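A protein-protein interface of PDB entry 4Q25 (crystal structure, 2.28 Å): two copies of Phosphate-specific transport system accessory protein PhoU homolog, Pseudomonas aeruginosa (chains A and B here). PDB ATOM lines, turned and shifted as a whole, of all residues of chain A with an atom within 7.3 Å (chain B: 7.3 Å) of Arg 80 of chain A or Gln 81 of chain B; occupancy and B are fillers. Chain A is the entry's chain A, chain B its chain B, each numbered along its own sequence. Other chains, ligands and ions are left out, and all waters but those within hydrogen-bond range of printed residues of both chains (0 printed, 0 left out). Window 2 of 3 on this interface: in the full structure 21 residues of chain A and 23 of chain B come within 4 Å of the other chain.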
ATOM      1  N   SER A  12      13.385 -10.966   8.600  1.00  0.00           N
ATOM      2  CA  SER A  12      14.358 -11.976   8.222  1.00  0.00           C
ATOM      3  C   SER A  12      15.411 -12.143   9.274  1.00  0.00           C
ATOM      4  O   SER A  12      15.411 -11.470  10.301  1.00  0.00           O
ATOM      5  CB  SER A  12      15.067 -11.604   6.923  1.00  0.00           C
ATOM      6  OG  SER A  12      15.821 -10.422   7.089  1.00  0.00           O
ATOM      7  N   PHE A  15      15.118 -15.483  10.033  1.00  0.00           N
ATOM      8  CA  PHE A  15      14.415 -16.455   9.224  1.00  0.00           C
ATOM      9  C   PHE A  15      15.413 -17.480   8.816  1.00  0.00           C
ATOM     10  O   PHE A  15      15.092 -18.601   8.487  1.00  0.00           O
ATOM     11  CB  PHE A  15      13.873 -15.831   7.957  1.00  0.00           C
ATOM     12  CG  PHE A  15      13.204 -16.811   7.061  1.00  0.00           C
ATOM     13  CD1 PHE A  15      11.918 -17.221   7.301  1.00  0.00           C
ATOM     14  CD2 PHE A  15      13.860 -17.310   5.959  1.00  0.00           C
ATOM     15  CE1 PHE A  15      11.296 -18.106   6.455  1.00  0.00           C
ATOM     16  CE2 PHE A  15      13.245 -18.201   5.119  1.00  0.00           C
ATOM     17  CZ  PHE A  15      11.964 -18.604   5.367  1.00  0.00           C
ATOM     18  N   ARG A  75       5.527 -23.826   8.429  1.00  0.00           N
ATOM     19  CA  ARG A  75       5.584 -22.630   9.216  1.00  0.00           C
ATOM     20  C   ARG A  75       6.533 -21.618   8.623  1.00  0.00           C
ATOM     21  O   ARG A  75       6.219 -20.428   8.486  1.00  0.00           O
ATOM     22  CB  ARG A  75       5.944 -22.984  10.631  1.00  0.00           C
ATOM     23  CG  ARG A  75       5.091 -24.103  11.169  1.00  0.00           C
ATOM     24  CD  ARG A  75       5.171 -24.251  12.668  1.00  0.00           C
ATOM     25  NE  ARG A  75       6.540 -24.314  13.141  1.00  0.00           N
ATOM     26  CZ  ARG A  75       7.159 -25.425  13.503  1.00  0.00           C
ATOM     27  NH1 ARG A  75       6.537 -26.575  13.453  1.00  0.00           N
ATOM     28  NH2 ARG A  75       8.401 -25.371  13.924  1.00  0.00           N
ATOM     29  N   ILE A  76       7.668 -22.103   8.178  1.00  0.00           N
ATOM     30  CA  ILE A  76       8.625 -21.221   7.626  1.00  0.00           C
ATOM     31  C   ILE A  76       8.047 -20.557   6.418  1.00  0.00           C
ATOM     32  O   ILE A  76       8.198 -19.386   6.250  1.00  0.00           O
ATOM     33  CB  ILE A  76       9.886 -21.961   7.161  1.00  0.00           C
ATOM     34  CG1 ILE A  76      10.786 -22.287   8.317  1.00  0.00           C
ATOM     35  CG2 ILE A  76      10.703 -21.111   6.217  1.00  0.00           C
ATOM     36  CD1 ILE A  76      11.963 -23.127   7.910  1.00  0.00           C
ATOM     37  N   LEU A  77       7.399 -21.302   5.556  1.00  0.00           N
ATOM     38  CA  LEU A  77       6.878 -20.722   4.341  1.00  0.00           C
ATOM     39  C   LEU A  77       5.774 -19.726   4.629  1.00  0.00           C
ATOM     40  O   LEU A  77       5.626 -18.742   3.958  1.00  0.00           O
ATOM     41  CB  LEU A  77       6.406 -21.786   3.378  1.00  0.00           C
ATOM     42  CG  LEU A  77       7.450 -22.491   2.532  1.00  0.00           C
ATOM     43  CD1 LEU A  77       6.810 -23.415   1.545  1.00  0.00           C
ATOM     44  CD2 LEU A  77       8.365 -21.539   1.803  1.00  0.00           C
ATOM     45  N   ALA A  78       4.980 -20.028   5.629  1.00  0.00           N
ATOM     46  CA  ALA A  78       3.847 -19.239   5.978  1.00  0.00           C
ATOM     47  C   ALA A  78       4.329 -17.874   6.304  1.00  0.00           C
ATOM     48  O   ALA A  78       3.696 -16.921   5.938  1.00  0.00           O
ATOM     49  CB  ALA A  78       3.124 -19.830   7.150  1.00  0.00           C
ATOM     50  N   ARG A  79       5.482 -17.712   6.923  1.00  0.00           N
ATOM     51  CA  ARG A  79       5.995 -16.371   7.203  1.00  0.00           C
ATOM     52  C   ARG A  79       6.671 -15.758   5.994  1.00  0.00           C
ATOM     53  O   ARG A  79       7.868 -15.681   5.910  1.00  0.00           O
ATOM     54  CB  ARG A  79       7.015 -16.390   8.320  1.00  0.00           C
ATOM     55  CG  ARG A  79       6.656 -17.279   9.478  1.00  0.00           C
ATOM     56  CD  ARG A  79       7.853 -17.379  10.382  1.00  0.00           C
ATOM     57  NE  ARG A  79       7.798 -18.556  11.227  1.00  0.00           N
ATOM     58  CZ  ARG A  79       7.133 -18.611  12.365  1.00  0.00           C
ATOM     59  NH1 ARG A  79       6.462 -17.552  12.780  1.00  0.00           N
ATOM     60  NH2 ARG A  79       7.127 -19.718  13.081  1.00  0.00           N
ATOM     61  N   ARG A  80       5.847 -15.333   5.057  1.00  0.00           N
ATOM     62  CA  ARG A  80       6.126 -14.229   4.167  1.00  0.00           C
ATOM     63  C   ARG A  80       6.938 -14.892   3.079  1.00  0.00           C
ATOM     64  O   ARG A  80       7.560 -15.893   3.325  1.00  0.00           O
ATOM     65  CB  ARG A  80       6.872 -13.080   4.891  1.00  0.00           C
ATOM     66  CG  ARG A  80       6.063 -12.337   5.974  1.00  0.00           C
ATOM     67  CD  ARG A  80       6.782 -11.169   6.657  1.00  0.00           C
ATOM     68  NE  ARG A  80       5.976 -10.558   7.722  1.00  0.00           N
ATOM     69  CZ  ARG A  80       6.383  -9.605   8.558  1.00  0.00           C
ATOM     70  NH1 ARG A  80       7.602  -9.098   8.491  1.00  0.00           N
ATOM     71  NH2 ARG A  80       5.549  -9.139   9.469  1.00  0.00           N
ATOM     72  N   GLN A  81       6.957 -14.344   1.888  1.00  0.00           N
ATOM     73  CA  GLN A  81       7.529 -15.081   0.801  1.00  0.00           C
ATOM     74  C   GLN A  81       9.043 -15.177   0.869  1.00  0.00           C
ATOM     75  O   GLN A  81       9.720 -14.211   1.127  1.00  0.00           O
ATOM     76  CB  GLN A  81       7.030 -14.539  -0.537  1.00  0.00           C
ATOM     77  CG  GLN A  81       7.752 -13.345  -1.085  1.00  0.00           C
ATOM     78  CD  GLN A  81       6.874 -12.528  -2.008  1.00  0.00           C
ATOM     79  OE1 GLN A  81       6.347 -11.501  -1.617  1.00  0.00           O
ATOM     80  NE2 GLN A  81       6.719 -12.982  -3.238  1.00  0.00           N
ATOM     81  N   PRO A  82       9.555 -16.373   0.613  1.00  0.00           N
ATOM     82  CA  PRO A  82      10.969 -16.665   0.539  1.00  0.00           C
ATOM     83  C   PRO A  82      11.518 -16.200  -0.785  1.00  0.00           C
ATOM     84  O   PRO A  82      10.826 -16.184  -1.769  1.00  0.00           O
ATOM     85  CB  PRO A  82      10.942 -18.165   0.489  1.00  0.00           C
ATOM     86  CG  PRO A  82       9.635 -18.403  -0.193  1.00  0.00           C
ATOM     87  CD  PRO A  82       8.704 -17.351   0.342  1.00  0.00           C
ATOM     88  N   ALA A  83      12.784 -15.867  -0.802  1.00  0.00           N
ATOM     89  CA  ALA A  83      13.485 -15.548  -2.018  1.00  0.00           C
ATOM     90  C   ALA A  83      13.663 -16.821  -2.780  1.00  0.00           C
ATOM     91  O   ALA A  83      13.478 -17.858  -2.255  1.00  0.00           O
ATOM     92  CB  ALA A  83      14.833 -14.978  -1.681  1.00  0.00           C
ATOM     93  N   ILE B  76       3.160 -21.633  -7.539  1.00  0.00           N
ATOM     94  CA  ILE B  76       2.206 -21.173  -6.537  1.00  0.00           C
ATOM     95  C   ILE B  76       2.887 -20.865  -5.224  1.00  0.00           C
ATOM     96  O   ILE B  76       2.581 -19.909  -4.594  1.00  0.00           O
ATOM     97  CB  ILE B  76       1.079 -22.185  -6.298  1.00  0.00           C
ATOM     98  CG1 ILE B  76       0.155 -22.242  -7.501  1.00  0.00           C
ATOM     99  CG2 ILE B  76       0.294 -21.816  -5.068  1.00  0.00           C
ATOM    100  CD1 ILE B  76      -0.932 -23.269  -7.408  1.00  0.00           C
ATOM    101  N   LEU B  77       3.813 -21.704  -4.838  1.00  0.00           N
ATOM    102  CA  LEU B  77       4.650 -21.487  -3.682  1.00  0.00           C
ATOM    103  C   LEU B  77       5.627 -20.338  -3.831  1.00  0.00           C
ATOM    104  O   LEU B  77       6.021 -19.748  -2.865  1.00  0.00           O
ATOM    105  CB  LEU B  77       5.382 -22.752  -3.320  1.00  0.00           C
ATOM    106  CG  LEU B  77       4.520 -23.949  -2.977  1.00  0.00           C
ATOM    107  CD1 LEU B  77       5.411 -25.097  -2.594  1.00  0.00           C
ATOM    108  CD2 LEU B  77       3.556 -23.637  -1.870  1.00  0.00           C
ATOM    109  N   ALA B  78       6.030 -20.032  -5.043  1.00  0.00           N
ATOM    110  CA  ALA B  78       6.780 -18.822  -5.295  1.00  0.00           C
ATOM    111  C   ALA B  78       5.965 -17.585  -4.994  1.00  0.00           C
ATOM    112  O   ALA B  78       6.508 -16.572  -4.608  1.00  0.00           O
ATOM    113  CB  ALA B  78       7.292 -18.790  -6.707  1.00  0.00           C
ATOM    114  N   ARG B  79       4.663 -17.654  -5.174  1.00  0.00           N
ATOM    115  CA  ARG B  79       3.954 -16.422  -5.396  1.00  0.00           C
ATOM    116  C   ARG B  79       3.590 -15.718  -4.106  1.00  0.00           C
ATOM    117  O   ARG B  79       4.093 -14.656  -3.820  1.00  0.00           O
ATOM    118  CB  ARG B  79       2.696 -16.683  -6.206  1.00  0.00           C
ATOM    119  CG  ARG B  79       2.852 -16.320  -7.656  1.00  0.00           C
ATOM    120  CD  ARG B  79       3.955 -15.289  -7.738  1.00  0.00           C
ATOM    121  NE  ARG B  79       4.736 -15.343  -8.971  1.00  0.00           N
ATOM    122  CZ  ARG B  79       5.601 -14.402  -9.324  1.00  0.00           C
ATOM    123  NH1 ARG B  79       5.793 -13.354  -8.540  1.00  0.00           N
ATOM    124  NH2 ARG B  79       6.263 -14.502 -10.459  1.00  0.00           N
ATOM    125  N   ARG B  80       2.763 -16.320  -3.287  1.00  0.00           N
ATOM    126  CA  ARG B  80       1.990 -15.498  -2.375  1.00  0.00           C
ATOM    127  C   ARG B  80       2.802 -15.419  -1.132  1.00  0.00           C
ATOM    128  O   ARG B  80       3.973 -15.748  -1.146  1.00  0.00           O
ATOM    129  CB  ARG B  80       0.587 -16.027  -2.114  1.00  0.00           C
ATOM    130  CG  ARG B  80      -0.347 -15.908  -3.309  1.00  0.00           C
ATOM    131  CD  ARG B  80      -1.757 -15.430  -2.966  1.00  0.00           C
ATOM    132  NE  ARG B  80      -2.453 -16.174  -1.914  1.00  0.00           N
ATOM    133  CZ  ARG B  80      -3.474 -15.672  -1.238  1.00  0.00           C
ATOM    134  NH1 ARG B  80      -3.862 -14.454  -1.517  1.00  0.00           N
ATOM    135  NH2 ARG B  80      -4.090 -16.354  -0.291  1.00  0.00           N
ATOM    136  N   GLN B  81       2.192 -14.974  -0.053  1.00  0.00           N
ATOM    137  CA  GLN B  81       2.348 -15.734   1.161  1.00  0.00           C
ATOM    138  C   GLN B  81       1.098 -16.385   1.723  1.00  0.00           C
ATOM    139  O   GLN B  81       0.194 -15.778   2.295  1.00  0.00           O
ATOM    140  CB  GLN B  81       3.084 -14.915   2.217  1.00  0.00           C
ATOM    141  CG  GLN B  81       2.871 -13.427   2.155  1.00  0.00           C
ATOM    142  CD  GLN B  81       2.836 -12.892   3.551  1.00  0.00           C
ATOM    143  OE1 GLN B  81       3.185 -13.622   4.482  1.00  0.00           O
ATOM    144  NE2 GLN B  81       2.406 -11.638   3.725  1.00  0.00           N
ATOM    145  N   PRO B  82       1.124 -17.682   1.593  1.00  0.00           N
ATOM    146  CA  PRO B  82      -0.065 -18.463   1.794  1.00  0.00           C
ATOM    147  C   PRO B  82      -0.293 -18.612   3.281  1.00  0.00           C
ATOM    148  O   PRO B  82       0.656 -18.557   4.037  1.00  0.00           O
ATOM    149  CB  PRO B  82       0.301 -19.759   1.126  1.00  0.00           C
ATOM    150  CG  PRO B  82       1.111 -19.327  -0.035  1.00  0.00           C
ATOM    151  CD  PRO B  82       1.843 -18.096   0.387  1.00  0.00           C
ATOM    152  N   ALA B  83      -1.535 -18.815   3.675  1.00  0.00           N
ATOM    153  CA  ALA B  83      -1.833 -19.404   4.947  1.00  0.00           C
ATOM    154  C   ALA B  83      -1.278 -20.807   5.028  1.00  0.00           C
ATOM    155  O   ALA B  83      -1.130 -21.487   4.061  1.00  0.00           O
ATOM    156  CB  ALA B  83      -3.317 -19.432   5.151  1.00  0.00           C
ATOM    157  N   ALA B  84      -0.911 -21.192   6.217  1.00  0.00           N
ATOM    158  CA  ALA B  84      -0.484 -22.534   6.479  1.00  0.00           C
ATOM    159  C   ALA B  84      -1.354 -23.596   5.809  1.00  0.00           C
ATOM    160  O   ALA B  84      -0.842 -24.533   5.224  1.00  0.00           O
ATOM    161  CB  ALA B  84      -0.453 -22.758   7.970  1.00  0.00           C
ATOM    162  N   ASP B  86      -3.251 -23.478   3.282  1.00  0.00           N
ATOM    163  CA  ASP B  86      -3.013 -23.481   1.838  1.00  0.00           C
ATOM    164  C   ASP B  86      -1.681 -24.137   1.458  1.00  0.00           C
ATOM    165  O   ASP B  86      -1.605 -24.821   0.450  1.00  0.00           O
ATOM    166  CB  ASP B  86      -3.043 -22.043   1.274  1.00  0.00           C
ATOM    167  CG  ASP B  86      -4.438 -21.486   1.173  1.00  0.00           C
ATOM    168  OD1 ASP B  86      -5.417 -22.268   1.166  1.00  0.00           O
ATOM    169  OD2 ASP B  86      -4.566 -20.255   1.095  1.00  0.00           O
ATOM    170  N   LEU B  87      -0.637 -23.891   2.246  1.00  0.00           N
ATOM    171  CA  LEU B  87       0.655 -24.549   2.032  1.00  0.00           C
ATOM    172  C   LEU B  87       0.512 -26.087   2.110  1.00  0.00           C
ATOM    173  O   LEU B  87       0.973 -26.818   1.238  1.00  0.00           O
ATOM    174  CB  LEU B  87       1.669 -24.085   3.063  1.00  0.00           C
ATOM    175  CG  LEU B  87       2.143 -22.619   3.100  1.00  0.00           C
ATOM    176  CD1 LEU B  87       3.044 -22.289   4.276  1.00  0.00           C
ATOM    177  CD2 LEU B  87       2.812 -22.225   1.821  1.00  0.00           C
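Of the 11 printed residues of chain B, 6 touch a printed residue of chain A. Along chain B the printed residues that touch a printed residue of chain A span positions 78 to 87. Among the printed residues, 9 pairs touch across the chains. Among the printed residues, no Asp or Glu carboxylate lies within 4 Å of a Lys or Arg side-chain nitrogen of the other chain.
Of the printed residues of chain B, Ala 78 of chain A touches Gln 81 (3.6 Å), Pro 82 (3.8 Å) and Leu 87 (3.3 Å). Of the printed residues of chain B, Arg 80 of chain A touches Gln 81 (3.0 Å). Printed residues of chain A within 4 Å of Ala 78 of chain B: Gln 81 (3.8 Å). The nearest residue of chain B that does not touch Arg 80 of chain A is Arg 80 of chain B (5.2 Å). The nearest residue of chain A that does not touch Gln 81 of chain B is Arg 79 of chain A (4.4 Å).
The backbone NH (N) of Arg 80 of chain A lies close to the side-chain amide oxygen (OE1) of Gln 81 of chain B (3.2 Å). The side-chain amide nitrogen (NE2) of Gln 81 of chain A sits at hydrogen-bond distance from the backbone carbonyl oxygen (O) of Arg 79 of chain B.
Among the printed residues, merely in contact across the chains: Ala 78 of chain A with Leu 87 of chain B (3.3 Å), Gln 81 of chain A with Arg 80 of chain B (3.3 Å), Leu 77 of chain A with Leu 87 of chain B (3.5 Å), Ala 78 of chain A with Gln 81 of chain B (3.6 Å), Ala 78 of chain A with Pro 82 of chain B (3.8 Å), Gln 81 of chain A with Ala 78 of chain B (3.8 Å) and Gln 81 of chain A with Gln 81 of chain B (3.9 Å).
Ala 78 of chain A touches Gln 81 of chain B, and with the chains exchanged Gln 81 of chain A touches Ala 78 of chain B. Ala 78 of chain A touches Pro 82 of chain B, but with the chains exchanged Pro 82 of chain A does not touch Ala 78 of chain B (5.2 Å). Arg 80 of chain A touches Gln 81 of chain B, and with the chains exchanged Gln 81 of chain A touches Arg 80 of chain B. Gln 81 of chain A touches Arg 79 of chain B, but with the chains exchanged Arg 79 of chain A does not touch Gln 81 of chain B (4.4 Å). Positions printed for both chains: 76, 77, 78, 79, 80, 81, 82 and 83.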
